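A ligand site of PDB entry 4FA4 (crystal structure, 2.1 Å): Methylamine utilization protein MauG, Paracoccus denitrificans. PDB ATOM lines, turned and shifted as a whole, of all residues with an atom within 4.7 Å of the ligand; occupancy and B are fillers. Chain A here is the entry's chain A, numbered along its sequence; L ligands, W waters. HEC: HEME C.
SG of Cys 34 is in hydrogen-bond range of NH2 of Arg 45 (3.2 Å). The backbone carbonyl oxygen of Pro 68 sits at hydrogen-bond distance from a ring nitrogen (ND1) of His 35 (3.1 Å). The backbone NH (N) of Arg 96 is in hydrogen-bond range of the backbone carbonyl oxygen (O) of Gln 91. NH2 of Arg 96 is in salt-bridge range of OD2 of Asp 94 (2.8 Å). The guanidinium group of Arg 65 lies within salt-bridge range of the side-chain carboxylate of Asp 94 (2.7 Å). The side-chain hydroxyl (OG) of Ser 54 is in hydrogen-bond range of the side-chain hydroxyl (OG1) of Thr 67 (2.6 Å). The backbone NH (N) of Met 114 lies close to the side-chain amide nitrogen (NE2) of Gln 29, at 3.5 Å. The side-chain amide oxygen of Gln 163 sits close to the backbone carbonyl oxygen of Leu 159, 3.4 Å away.
SG of Cys 31 is covalently linked to CAB of the ligand (1.8 Å). The side-chain sulfur of Cys 34 is bonded to a carbon (CAC) of the ligand (1.8 Å). An iron atom (FE) of the ligand is bound by a ring nitrogen (NE2) of His 35 (1.9 Å). NH2 of Arg 96 lies within salt-bridge range of O1D of the ligand (2.7 Å). The backbone NH (N) of Phe 92 sits at hydrogen-bond distance from an oxygen (O2A) of the ligand (2.7 Å). An oxygen (O1D) of the ligand is in salt-bridge range of the guanidinium group (NH1) of Arg 65, 3.0 Å away. N of Trp 93 sits close to O2D of the ligand, at 3.0 Å. O1A of the ligand lies within salt-bridge range of NZ of Lys 265.
Water W2 bridges an oxygen (O2A) of the ligand (2.9 Å) and the side-chain amino group (NZ) of Lys 265 (3.5 Å). Water W1 lies within hydrogen-bond range of the backbone carbonyl oxygen (O) of Arg 65 (2.7 Å) and the backbone NH (N) of Ser 54 (2.9 Å).
A nitrogen (NA) of the ligand sits close to the side-chain amide nitrogen (NE2) of Gln 103 (3.1 Å). Gln 29 touches the ligand (NE2 to CMC, 3.2 Å). Ser 30 touches the ligand. Ser 54 touches the ligand (CB to CAC, 3.5 Å). Val 55 touches the ligand (O to CBC, 3.8 Å). Asn 66 touches the ligand (O to CAD, 3.8 Å). Thr 67 touches the ligand (OG1 to CHD, 3.1 Å). CD of Pro 68 touches C3D of the ligand (3.3 Å). CD2 of Leu 70 touches C4A of the ligand, at 3.5 Å. NE2 of Gln 91 touches CGA of the ligand (3.4 Å). Leu 100 touches the ligand (CD2 to CMA, 3.3 Å). Ala 104 touches the ligand (O to CBB, 3.4 Å). Pro 107 touches the ligand. Met 108 touches the ligand. OE2 of Glu 113 touches CHD of the ligand (3.8 Å). CG of Met 114 touches CMC of the ligand, at 3.7 Å. CD1 of Leu 159 touches CBB of the ligand, at 3.98 Å. Gln 163 touches the ligand. Hydrophobic or aromatic side chains within 4 Å of the ligand: His 35, Pro 68, Leu 70, Phe 92, Trp 93, Leu 100, Pro 107, Met 108, Met 114 and Leu 159. Of the 32 residues printed, 26 come within 4 Å of the ligand. Along chain A the residues within 4 Å of the ligand span positions 29 to 265.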
ATOM      1  N   GLN A  29     -20.150  -6.879 -40.013  1.00  0.00           N
ATOM      2  CA  GLN A  29     -20.544  -7.690 -38.854  1.00  0.00           C
ATOM      3  C   GLN A  29     -21.583  -8.792 -39.074  1.00  0.00           C
ATOM      4  O   GLN A  29     -22.459  -8.676 -39.936  1.00  0.00           O
ATOM      5  CB  GLN A  29     -20.832  -6.838 -37.615  1.00  0.00           C
ATOM      6  CG  GLN A  29     -22.215  -6.355 -37.392  1.00  0.00           C
ATOM      7  CD  GLN A  29     -22.300  -5.550 -36.112  1.00  0.00           C
ATOM      8  OE1 GLN A  29     -21.273  -5.182 -35.511  1.00  0.00           O
ATOM      9  NE2 GLN A  29     -23.530  -5.273 -35.674  1.00  0.00           N
ATOM     10  N   SER A  30     -21.446  -9.869 -38.290  1.00  0.00           N
ATOM     11  CA  SER A  30     -22.343 -10.996 -38.366  1.00  0.00           C
ATOM     12  C   SER A  30     -22.858 -11.160 -36.958  1.00  0.00           C
ATOM     13  O   SER A  30     -22.323 -10.493 -36.035  1.00  0.00           O
ATOM     14  CB  SER A  30     -21.598 -12.243 -38.815  1.00  0.00           C
ATOM     15  OG  SER A  30     -20.699 -12.641 -37.800  1.00  0.00           O
ATOM     16  N   CYS A  31     -23.880 -12.002 -36.772  1.00  0.00           N
ATOM     17  CA  CYS A  31     -24.319 -12.351 -35.408  1.00  0.00           C
ATOM     18  C   CYS A  31     -23.094 -12.722 -34.583  1.00  0.00           C
ATOM     19  O   CYS A  31     -22.913 -12.225 -33.474  1.00  0.00           O
ATOM     20  CB  CYS A  31     -25.290 -13.538 -35.386  1.00  0.00           C
ATOM     21  SG  CYS A  31     -26.617 -13.518 -36.595  1.00  0.00           S
ATOM     22  N   CYS A  34     -20.902 -10.171 -32.511  1.00  0.00           N
ATOM     23  CA  CYS A  34     -21.271  -9.792 -31.168  1.00  0.00           C
ATOM     24  C   CYS A  34     -21.545 -11.000 -30.344  1.00  0.00           C
ATOM     25  O   CYS A  34     -21.413 -10.952 -29.110  1.00  0.00           O
ATOM     26  CB  CYS A  34     -22.509  -8.970 -31.158  1.00  0.00           C
ATOM     27  SG  CYS A  34     -22.270  -7.372 -31.786  1.00  0.00           S
ATOM     28  N   HIS A  35     -22.052 -12.061 -30.989  1.00  0.00           N
ATOM     29  CA  HIS A  35     -22.298 -13.231 -30.191  1.00  0.00           C
ATOM     30  C   HIS A  35     -21.205 -14.225 -30.516  1.00  0.00           C
ATOM     31  O   HIS A  35     -21.446 -15.205 -31.231  1.00  0.00           O
ATOM     32  CB  HIS A  35     -23.685 -13.806 -30.441  1.00  0.00           C
ATOM     33  CG  HIS A  35     -24.805 -12.859 -30.088  1.00  0.00           C
ATOM     34  ND1 HIS A  35     -25.282 -12.716 -28.801  1.00  0.00           N
ATOM     35  CD2 HIS A  35     -25.559 -12.037 -30.852  1.00  0.00           C
ATOM     36  CE1 HIS A  35     -26.305 -11.875 -28.797  1.00  0.00           C
ATOM     37  NE2 HIS A  35     -26.490 -11.442 -30.036  1.00  0.00           N
ATOM     38  N   ARG A  45     -15.303  -7.649 -27.805  1.00  0.00           N
ATOM     39  CA  ARG A  45     -14.781  -6.377 -28.390  1.00  0.00           C
ATOM     40  C   ARG A  45     -14.909  -5.130 -27.474  1.00  0.00           C
ATOM     41  O   ARG A  45     -16.001  -4.776 -27.024  1.00  0.00           O
ATOM     42  CB  ARG A  45     -15.437  -6.079 -29.741  1.00  0.00           C
ATOM     43  CG  ARG A  45     -15.153  -7.097 -30.873  1.00  0.00           C
ATOM     44  CD  ARG A  45     -16.028  -6.819 -32.091  1.00  0.00           C
ATOM     45  NE  ARG A  45     -17.423  -6.639 -31.650  1.00  0.00           N
ATOM     46  CZ  ARG A  45     -18.267  -5.730 -32.136  1.00  0.00           C
ATOM     47  NH1 ARG A  45     -17.855  -4.923 -33.116  1.00  0.00           N
ATOM     48  NH2 ARG A  45     -19.534  -5.671 -31.663  1.00  0.00           N
ATOM     49  N   SER A  54     -22.025  -3.391 -26.946  1.00  0.00           N
ATOM     50  CA  SER A  54     -21.393  -3.662 -28.243  1.00  0.00           C
ATOM     51  C   SER A  54     -21.577  -2.519 -29.259  1.00  0.00           C
ATOM     52  O   SER A  54     -22.547  -1.718 -29.186  1.00  0.00           O
ATOM     53  CB  SER A  54     -22.007  -4.923 -28.840  1.00  0.00           C
ATOM     54  OG  SER A  54     -21.844  -5.990 -27.929  1.00  0.00           O
ATOM     55  N   VAL A  55     -20.670  -2.513 -30.247  1.00  0.00           N
ATOM     56  CA  VAL A  55     -20.619  -1.496 -31.285  1.00  0.00           C
ATOM     57  C   VAL A  55     -21.225  -2.034 -32.564  1.00  0.00           C
ATOM     58  O   VAL A  55     -20.807  -3.077 -33.048  1.00  0.00           O
ATOM     59  CB  VAL A  55     -19.144  -1.116 -31.506  1.00  0.00           C
ATOM     60  CG1 VAL A  55     -18.976  -0.063 -32.611  1.00  0.00           C
ATOM     61  CG2 VAL A  55     -18.551  -0.658 -30.146  1.00  0.00           C
ATOM     62  N   GLY A  56     -22.197  -1.331 -33.117  1.00  0.00           N
ATOM     63  CA  GLY A  56     -22.797  -1.785 -34.373  1.00  0.00           C
ATOM     64  C   GLY A  56     -21.853  -1.777 -35.574  1.00  0.00           C
ATOM     65  O   GLY A  56     -20.668  -1.391 -35.454  1.00  0.00           O
ATOM     66  N   ARG A  65     -27.508  -1.917 -23.882  1.00  0.00           N
ATOM     67  CA  ARG A  65     -27.535  -3.133 -23.112  1.00  0.00           C
ATOM     68  C   ARG A  65     -26.417  -4.047 -23.523  1.00  0.00           C
ATOM     69  O   ARG A  65     -25.944  -4.020 -24.672  1.00  0.00           O
ATOM     70  CB  ARG A  65     -28.879  -3.834 -23.275  1.00  0.00           C
ATOM     71  CG  ARG A  65     -30.054  -3.001 -22.778  1.00  0.00           C
ATOM     72  CD  ARG A  65     -31.307  -3.801 -22.872  1.00  0.00           C
ATOM     73  NE  ARG A  65     -32.456  -3.033 -22.345  1.00  0.00           N
ATOM     74  CZ  ARG A  65     -33.705  -3.193 -22.778  1.00  0.00           C
ATOM     75  NH1 ARG A  65     -33.975  -4.085 -23.720  1.00  0.00           N
ATOM     76  NH2 ARG A  65     -34.695  -2.491 -22.257  1.00  0.00           N
ATOM     77  N   ASN A  66     -25.994  -4.865 -22.565  1.00  0.00           N
ATOM     78  CA  ASN A  66     -24.957  -5.862 -22.684  1.00  0.00           C
ATOM     79  C   ASN A  66     -25.472  -7.024 -23.536  1.00  0.00           C
ATOM     80  O   ASN A  66     -26.677  -7.433 -23.455  1.00  0.00           O
ATOM     81  CB  ASN A  66     -24.620  -6.360 -21.291  1.00  0.00           C
ATOM     82  CG  ASN A  66     -23.520  -7.387 -21.285  1.00  0.00           C
ATOM     83  OD1 ASN A  66     -23.708  -8.560 -20.810  1.00  0.00           O
ATOM     84  ND2 ASN A  66     -22.334  -6.966 -21.774  1.00  0.00           N
ATOM     85  N   THR A  67     -24.593  -7.505 -24.387  1.00  0.00           N
ATOM     86  CA  THR A  67     -24.892  -8.575 -25.296  1.00  0.00           C
ATOM     87  C   THR A  67     -24.953  -9.866 -24.476  1.00  0.00           C
ATOM     88  O   THR A  67     -23.961 -10.278 -23.876  1.00  0.00           O
ATOM     89  CB  THR A  67     -23.856  -8.607 -26.445  1.00  0.00           C
ATOM     90  OG1 THR A  67     -23.964  -7.397 -27.224  1.00  0.00           O
ATOM     91  CG2 THR A  67     -24.077  -9.855 -27.345  1.00  0.00           C
ATOM     92  N   PRO A  68     -26.148 -10.497 -24.395  1.00  0.00           N
ATOM     93  CA  PRO A  68     -26.246 -11.769 -23.711  1.00  0.00           C
ATOM     94  C   PRO A  68     -25.765 -12.981 -24.548  1.00  0.00           C
ATOM     95  O   PRO A  68     -25.733 -12.995 -25.797  1.00  0.00           O
ATOM     96  CB  PRO A  68     -27.743 -11.881 -23.381  1.00  0.00           C
ATOM     97  CG  PRO A  68     -28.388 -11.221 -24.536  1.00  0.00           C
ATOM     98  CD  PRO A  68     -27.461 -10.066 -24.916  1.00  0.00           C
ATOM     99  N   THR A  69     -25.394 -14.007 -23.831  1.00  0.00           N
ATOM    100  CA  THR A  69     -25.139 -15.264 -24.426  1.00  0.00           C
ATOM    101  C   THR A  69     -26.360 -15.763 -25.193  1.00  0.00           C
ATOM    102  O   THR A  69     -27.521 -15.439 -24.864  1.00  0.00           O
ATOM    103  CB  THR A  69     -24.859 -16.254 -23.360  1.00  0.00           C
ATOM    104  OG1 THR A  69     -24.476 -17.462 -23.998  1.00  0.00           O
ATOM    105  CG2 THR A  69     -26.178 -16.437 -22.434  1.00  0.00           C
ATOM    106  N   LEU A  70     -26.106 -16.520 -26.252  1.00  0.00           N
ATOM    107  CA  LEU A  70     -27.184 -17.217 -26.949  1.00  0.00           C
ATOM    108  C   LEU A  70     -27.295 -18.638 -26.391  1.00  0.00           C
ATOM    109  O   LEU A  70     -28.288 -19.298 -26.639  1.00  0.00           O
ATOM    110  CB  LEU A  70     -26.870 -17.276 -28.451  1.00  0.00           C
ATOM    111  CG  LEU A  70     -26.754 -15.888 -29.100  1.00  0.00           C
ATOM    112  CD1 LEU A  70     -26.863 -16.055 -30.536  1.00  0.00           C
ATOM    113  CD2 LEU A  70     -27.828 -14.892 -28.628  1.00  0.00           C
ATOM    114  N   ALA A  73     -30.545 -20.157 -24.738  1.00  0.00           N
ATOM    115  CA  ALA A  73     -31.634 -19.242 -24.974  1.00  0.00           C
ATOM    116  C   ALA A  73     -32.801 -20.012 -25.589  1.00  0.00           C
ATOM    117  O   ALA A  73     -33.981 -19.665 -25.389  1.00  0.00           O
ATOM    118  CB  ALA A  73     -31.198 -18.066 -25.851  1.00  0.00           C
ATOM    119  N   GLN A  91     -37.523 -13.077 -25.428  1.00  0.00           N
ATOM    120  CA  GLN A  91     -36.103 -12.884 -25.743  1.00  0.00           C
ATOM    121  C   GLN A  91     -35.801 -11.406 -25.597  1.00  0.00           C
ATOM    122  O   GLN A  91     -36.732 -10.598 -25.629  1.00  0.00           O
ATOM    123  CB  GLN A  91     -35.780 -13.357 -27.168  1.00  0.00           C
ATOM    124  CG  GLN A  91     -35.950 -14.854 -27.346  1.00  0.00           C
ATOM    125  CD  GLN A  91     -35.049 -15.729 -26.421  1.00  0.00           C
ATOM    126  OE1 GLN A  91     -35.411 -16.884 -26.059  1.00  0.00           O
ATOM    127  NE2 GLN A  91     -33.898 -15.210 -26.072  1.00  0.00           N
ATOM    128  N   PHE A  92     -34.508 -11.079 -25.493  1.00  0.00           N
ATOM    129  CA  PHE A  92     -34.044  -9.751 -25.027  1.00  0.00           C
ATOM    130  C   PHE A  92     -34.279  -9.609 -23.527  1.00  0.00           C
ATOM    131  O   PHE A  92     -35.171 -10.227 -22.942  1.00  0.00           O
ATOM    132  CB  PHE A  92     -34.756  -8.581 -25.701  1.00  0.00           C
ATOM    133  CG  PHE A  92     -34.424  -8.408 -27.138  1.00  0.00           C
ATOM    134  CD1 PHE A  92     -33.106  -8.262 -27.542  1.00  0.00           C
ATOM    135  CD2 PHE A  92     -35.435  -8.382 -28.106  1.00  0.00           C
ATOM    136  CE1 PHE A  92     -32.757  -8.098 -28.907  1.00  0.00           C
ATOM    137  CE2 PHE A  92     -35.114  -8.184 -29.433  1.00  0.00           C
ATOM    138  CZ  PHE A  92     -33.760  -8.058 -29.841  1.00  0.00           C
ATOM    139  N   TRP A  93     -33.486  -8.747 -22.940  1.00  0.00           N
ATOM    140  CA  TRP A  93     -33.531  -8.427 -21.529  1.00  0.00           C
ATOM    141  C   TRP A  93     -34.881  -7.892 -21.094  1.00  0.00           C
ATOM    142  O   TRP A  93     -35.242  -8.035 -19.931  1.00  0.00           O
ATOM    143  CB  TRP A  93     -32.482  -7.381 -21.211  1.00  0.00           C
ATOM    144  CG  TRP A  93     -31.088  -7.813 -21.220  1.00  0.00           C
ATOM    145  CD1 TRP A  93     -30.176  -7.562 -22.194  1.00  0.00           C
ATOM    146  CD2 TRP A  93     -30.390  -8.540 -20.187  1.00  0.00           C
ATOM    147  NE1 TRP A  93     -28.945  -8.070 -21.835  1.00  0.00           N
ATOM    148  CE2 TRP A  93     -29.049  -8.679 -20.610  1.00  0.00           C
ATOM    149  CE3 TRP A  93     -30.760  -9.064 -18.936  1.00  0.00           C
ATOM    150  CZ2 TRP A  93     -28.058  -9.335 -19.807  1.00  0.00           C
ATOM    151  CZ3 TRP A  93     -29.779  -9.734 -18.157  1.00  0.00           C
ATOM    152  CH2 TRP A  93     -28.458  -9.845 -18.591  1.00  0.00           C
ATOM    153  N   ASP A  94     -35.599  -7.292 -22.011  1.00  0.00           N
ATOM    154  CA  ASP A  94     -36.919  -6.771 -21.682  1.00  0.00           C
ATOM    155  C   ASP A  94     -38.040  -7.604 -22.260  1.00  0.00           C
ATOM    156  O   ASP A  94     -39.175  -7.208 -22.221  1.00  0.00           O
ATOM    157  CB  ASP A  94     -37.069  -5.310 -22.098  1.00  0.00           C
ATOM    158  CG  ASP A  94     -36.798  -5.066 -23.590  1.00  0.00           C
ATOM    159  OD1 ASP A  94     -36.654  -3.882 -23.976  1.00  0.00           O
ATOM    160  OD2 ASP A  94     -36.691  -6.022 -24.378  1.00  0.00           O
ATOM    161  N   ARG A  96     -39.023  -8.201 -25.202  1.00  0.00           N
ATOM    162  CA  ARG A  96     -39.841  -7.609 -26.221  1.00  0.00           C
ATOM    163  C   ARG A  96     -40.062  -8.482 -27.471  1.00  0.00           C
ATOM    164  O   ARG A  96     -40.981  -8.220 -28.228  1.00  0.00           O
ATOM    165  CB  ARG A  96     -39.342  -6.221 -26.548  1.00  0.00           C
ATOM    166  CG  ARG A  96     -37.981  -6.214 -27.231  1.00  0.00           C
ATOM    167  CD  ARG A  96     -37.586  -4.751 -27.641  1.00  0.00           C
ATOM    168  NE  ARG A  96     -36.288  -4.712 -28.362  1.00  0.00           N
ATOM    169  CZ  ARG A  96     -35.087  -4.833 -27.762  1.00  0.00           C
ATOM    170  NH1 ARG A  96     -33.958  -4.807 -28.461  1.00  0.00           N
ATOM    171  NH2 ARG A  96     -35.018  -5.008 -26.449  1.00  0.00           N
ATOM    172  N   LEU A 100     -37.208 -16.869 -30.377  1.00  0.00           N
ATOM    173  CA  LEU A 100     -35.908 -16.676 -31.085  1.00  0.00           C
ATOM    174  C   LEU A 100     -36.110 -16.258 -32.502  1.00  0.00           C
ATOM    175  O   LEU A 100     -35.325 -15.475 -33.041  1.00  0.00           O
ATOM    176  CB  LEU A 100     -35.090 -17.959 -31.091  1.00  0.00           C
ATOM    177  CG  LEU A 100     -34.493 -18.344 -29.763  1.00  0.00           C
ATOM    178  CD1 LEU A 100     -34.017 -19.863 -29.774  1.00  0.00           C
ATOM    179  CD2 LEU A 100     -33.386 -17.342 -29.417  1.00  0.00           C
ATOM    180  N   GLN A 103     -37.006 -12.726 -32.584  1.00  0.00           N
ATOM    181  CA  GLN A 103     -35.841 -11.952 -32.219  1.00  0.00           C
ATOM    182  C   GLN A 103     -34.800 -11.832 -33.364  1.00  0.00           C
ATOM    183  O   GLN A 103     -34.192 -10.756 -33.502  1.00  0.00           O
ATOM    184  CB  GLN A 103     -35.207 -12.529 -30.971  1.00  0.00           C
ATOM    185  CG  GLN A 103     -34.094 -11.639 -30.414  1.00  0.00           C
ATOM    186  CD  GLN A 103     -32.873 -11.629 -31.324  1.00  0.00           C
ATOM    187  OE1 GLN A 103     -32.650 -12.571 -32.112  1.00  0.00           O
ATOM    188  NE2 GLN A 103     -32.060 -10.570 -31.207  1.00  0.00           N
ATOM    189  N   ALA A 104     -34.612 -12.899 -34.171  1.00  0.00           N
ATOM    190  CA  ALA A 104     -33.522 -12.997 -35.161  1.00  0.00           C
ATOM    191  C   ALA A 104     -33.429 -11.867 -36.197  1.00  0.00           C
ATOM    192  O   ALA A 104     -32.338 -11.457 -36.603  1.00  0.00           O
ATOM    193  CB  ALA A 104     -33.529 -14.383 -35.885  1.00  0.00           C
ATOM    194  N   PRO A 107     -31.744  -7.663 -34.952  1.00  0.00           N
ATOM    195  CA  PRO A 107     -30.377  -7.099 -35.130  1.00  0.00           C
ATOM    196  C   PRO A 107     -29.981  -6.677 -36.542  1.00  0.00           C
ATOM    197  O   PRO A 107     -29.207  -5.762 -36.714  1.00  0.00           O
ATOM    198  CB  PRO A 107     -29.443  -8.239 -34.656  1.00  0.00           C
ATOM    199  CG  PRO A 107     -30.367  -9.355 -34.149  1.00  0.00           C
ATOM    200  CD  PRO A 107     -31.734  -8.793 -34.017  1.00  0.00           C
ATOM    201  N   MET A 108     -30.472  -7.404 -37.538  1.00  0.00           N
ATOM    202  CA  MET A 108     -30.251  -7.118 -38.935  1.00  0.00           C
ATOM    203  C   MET A 108     -30.648  -5.736 -39.416  1.00  0.00           C
ATOM    204  O   MET A 108     -29.983  -5.164 -40.267  1.00  0.00           O
ATOM    205  CB  MET A 108     -31.024  -8.120 -39.800  1.00  0.00           C
ATOM    206  CG  MET A 108     -30.430  -9.492 -39.730  1.00  0.00           C
ATOM    207  SD  MET A 108     -31.149 -10.610 -40.937  1.00  0.00           S
ATOM    208  CE  MET A 108     -30.958 -12.164 -40.039  1.00  0.00           C
ATOM    209  N   VAL A 112     -28.370   0.632 -34.834  1.00  0.00           N
ATOM    210  CA  VAL A 112     -27.210   0.618 -33.895  1.00  0.00           C
ATOM    211  C   VAL A 112     -26.421  -0.726 -33.894  1.00  0.00           C
ATOM    212  O   VAL A 112     -25.423  -0.888 -33.173  1.00  0.00           O
ATOM    213  CB  VAL A 112     -27.513   1.187 -32.432  1.00  0.00           C
ATOM    214  CG1 VAL A 112     -28.870   1.969 -32.324  1.00  0.00           C
ATOM    215  CG2 VAL A 112     -27.416   0.143 -31.409  1.00  0.00           C
ATOM    216  N   GLU A 113     -26.910  -1.678 -34.698  1.00  0.00           N
ATOM    217  CA  GLU A 113     -26.343  -3.014 -34.795  1.00  0.00           C
ATOM    218  C   GLU A 113     -25.991  -3.285 -36.233  1.00  0.00           C
ATOM    219  O   GLU A 113     -25.153  -2.605 -36.804  1.00  0.00           O
ATOM    220  CB  GLU A 113     -27.287  -4.067 -34.196  1.00  0.00           C
ATOM    221  CG  GLU A 113     -27.591  -3.751 -32.669  1.00  0.00           C
ATOM    222  CD  GLU A 113     -28.434  -4.842 -31.929  1.00  0.00           C
ATOM    223  OE1 GLU A 113     -29.181  -5.574 -32.613  1.00  0.00           O
ATOM    224  OE2 GLU A 113     -28.335  -4.993 -30.673  1.00  0.00           O
ATOM    225  N   MET A 114     -26.629  -4.258 -36.865  1.00  0.00           N
ATOM    226  CA  MET A 114     -26.154  -4.628 -38.178  1.00  0.00           C
ATOM    227  C   MET A 114     -26.539  -3.623 -39.254  1.00  0.00           C
ATOM    228  O   MET A 114     -25.844  -3.508 -40.274  1.00  0.00           O
ATOM    229  CB  MET A 114     -26.450  -6.073 -38.521  1.00  0.00           C
ATOM    230  CG  MET A 114     -25.884  -7.045 -37.476  1.00  0.00           C
ATOM    231  SD  MET A 114     -26.622  -8.701 -37.618  1.00  0.00           S
ATOM    232  CE  MET A 114     -25.949  -9.266 -39.153  1.00  0.00           C
ATOM    233  N   LEU A 159     -31.820 -18.970 -38.475  1.00  0.00           N
ATOM    234  CA  LEU A 159     -31.040 -18.568 -37.284  1.00  0.00           C
ATOM    235  C   LEU A 159     -31.589 -19.233 -35.976  1.00  0.00           C
ATOM    236  O   LEU A 159     -30.807 -19.745 -35.165  1.00  0.00           O
ATOM    237  CB  LEU A 159     -30.987 -17.040 -37.143  1.00  0.00           C
ATOM    238  CG  LEU A 159     -29.967 -16.522 -38.185  1.00  0.00           C
ATOM    239  CD1 LEU A 159     -30.313 -15.112 -38.552  1.00  0.00           C
ATOM    240  CD2 LEU A 159     -28.423 -16.655 -37.838  1.00  0.00           C
ATOM    241  N   GLN A 163     -29.953 -21.816 -33.394  1.00  0.00           N
ATOM    242  CA  GLN A 163     -29.753 -21.590 -31.929  1.00  0.00           C
ATOM    243  C   GLN A 163     -30.346 -22.688 -31.027  1.00  0.00           C
ATOM    244  O   GLN A 163     -30.056 -22.758 -29.814  1.00  0.00           O
ATOM    245  CB  GLN A 163     -30.243 -20.215 -31.505  1.00  0.00           C
ATOM    246  CG  GLN A 163     -29.399 -19.090 -32.001  1.00  0.00           C
ATOM    247  CD  GLN A 163     -30.082 -17.771 -31.849  1.00  0.00           C
ATOM    248  OE1 GLN A 163     -30.800 -17.321 -32.758  1.00  0.00           O
ATOM    249  NE2 GLN A 163     -29.862 -17.126 -30.711  1.00  0.00           N
ATOM    250  N   LYS A 265     -35.708  -9.668 -17.637  1.00  0.00           N
ATOM    251  CA  LYS A 265     -35.715 -11.137 -17.659  1.00  0.00           C
ATOM    252  C   LYS A 265     -34.580 -11.674 -16.837  1.00  0.00           C
ATOM    253  O   LYS A 265     -33.449 -11.241 -17.014  1.00  0.00           O
ATOM    254  CB  LYS A 265     -35.555 -11.638 -19.099  1.00  0.00           C
ATOM    255  CG  LYS A 265     -35.498 -13.144 -19.254  1.00  0.00           C
ATOM    256  CD  LYS A 265     -35.790 -13.521 -20.691  1.00  0.00           C
ATOM    257  CE  LYS A 265     -34.631 -13.130 -21.673  1.00  0.00           C
ATOM    258  NZ  LYS A 265     -33.226 -13.489 -21.244  1.00  0.00           N
HETATM  259 FE   HEC L   1     -27.947 -10.301 -30.574  1.00  0.00          FE
HETATM  260  CHA HEC L   1     -29.775 -10.058 -27.717  1.00  0.00           C
HETATM  261  CHB HEC L   1     -29.511 -13.199 -31.408  1.00  0.00           C
HETATM  262  CHC HEC L   1     -26.632 -10.091 -33.805  1.00  0.00           C
HETATM  263  CHD HEC L   1     -25.973  -7.774 -29.544  1.00  0.00           C
HETATM  264  NA  HEC L   1     -29.433 -11.439 -29.710  1.00  0.00           N
HETATM  265  C1A HEC L   1     -30.015 -11.263 -28.522  1.00  0.00           C
HETATM  266  C2A HEC L   1     -30.932 -12.364 -28.123  1.00  0.00           C
HETATM  267  C3A HEC L   1     -30.876 -13.232 -29.200  1.00  0.00           C
HETATM  268  C4A HEC L   1     -29.922 -12.592 -30.153  1.00  0.00           C
HETATM  269  CMA HEC L   1     -31.533 -14.553 -29.353  1.00  0.00           C
HETATM  270  CAA HEC L   1     -31.744 -12.517 -26.841  1.00  0.00           C
HETATM  271  CBA HEC L   1     -30.806 -13.226 -25.826  1.00  0.00           C
HETATM  272  CGA HEC L   1     -31.553 -13.238 -24.494  1.00  0.00           C
HETATM  273  O1A HEC L   1     -31.204 -14.005 -23.581  1.00  0.00           O
HETATM  274  O2A HEC L   1     -32.535 -12.464 -24.325  1.00  0.00           O
HETATM  275  NB  HEC L   1     -28.022 -11.470 -32.312  1.00  0.00           N
HETATM  276  C1B HEC L   1     -28.783 -12.557 -32.502  1.00  0.00           C
HETATM  277  C2B HEC L   1     -28.847 -13.070 -33.888  1.00  0.00           C
HETATM  278  C3B HEC L   1     -28.035 -12.166 -34.584  1.00  0.00           C
HETATM  279  C4B HEC L   1     -27.559 -11.203 -33.549  1.00  0.00           C
HETATM  280  CMB HEC L   1     -29.649 -14.286 -34.337  1.00  0.00           C
HETATM  281  CAB HEC L   1     -27.711 -12.149 -36.048  1.00  0.00           C
HETATM  282  CBB HEC L   1     -28.926 -11.787 -36.868  1.00  0.00           C
HETATM  283  NC  HEC L   1     -26.509  -9.112 -31.494  1.00  0.00           N
HETATM  284  C1C HEC L   1     -26.069  -9.174 -32.763  1.00  0.00           C
HETATM  285  C2C HEC L   1     -24.986  -8.209 -33.027  1.00  0.00           C
HETATM  286  C3C HEC L   1     -24.792  -7.536 -31.827  1.00  0.00           C
HETATM  287  C4C HEC L   1     -25.794  -8.158 -30.949  1.00  0.00           C
HETATM  288  CMC HEC L   1     -24.258  -8.073 -34.338  1.00  0.00           C
HETATM  289  CAC HEC L   1     -23.805  -6.423 -31.444  1.00  0.00           C
HETATM  290  CBC HEC L   1     -23.919  -5.197 -32.324  1.00  0.00           C
HETATM  291  ND  HEC L   1     -27.850  -9.116 -28.871  1.00  0.00           N
HETATM  292  C1D HEC L   1     -27.129  -8.050 -28.683  1.00  0.00           C
HETATM  293  C2D HEC L   1     -27.534  -7.196 -27.533  1.00  0.00           C
HETATM  294  C3D HEC L   1     -28.624  -7.846 -27.043  1.00  0.00           C
HETATM  295  C4D HEC L   1     -28.755  -9.016 -27.917  1.00  0.00           C
HETATM  296  CMD HEC L   1     -26.908  -5.900 -27.120  1.00  0.00           C
HETATM  297  CAD HEC L   1     -29.556  -7.508 -25.903  1.00  0.00           C
HETATM  298  CBD HEC L   1     -30.416  -6.406 -26.452  1.00  0.00           C
HETATM  299  CGD HEC L   1     -31.629  -6.112 -25.610  1.00  0.00           C
HETATM  300  O1D HEC L   1     -32.393  -5.186 -26.002  1.00  0.00           O
HETATM  301  O2D HEC L   1     -31.857  -6.780 -24.555  1.00  0.00           O
HETATM  302  O   HOH W   1     -24.882  -3.341 -27.089  1.00  0.00           O
HETATM  303  O   HOH W   2     -30.886 -11.159 -22.273  1.00  0.00           O
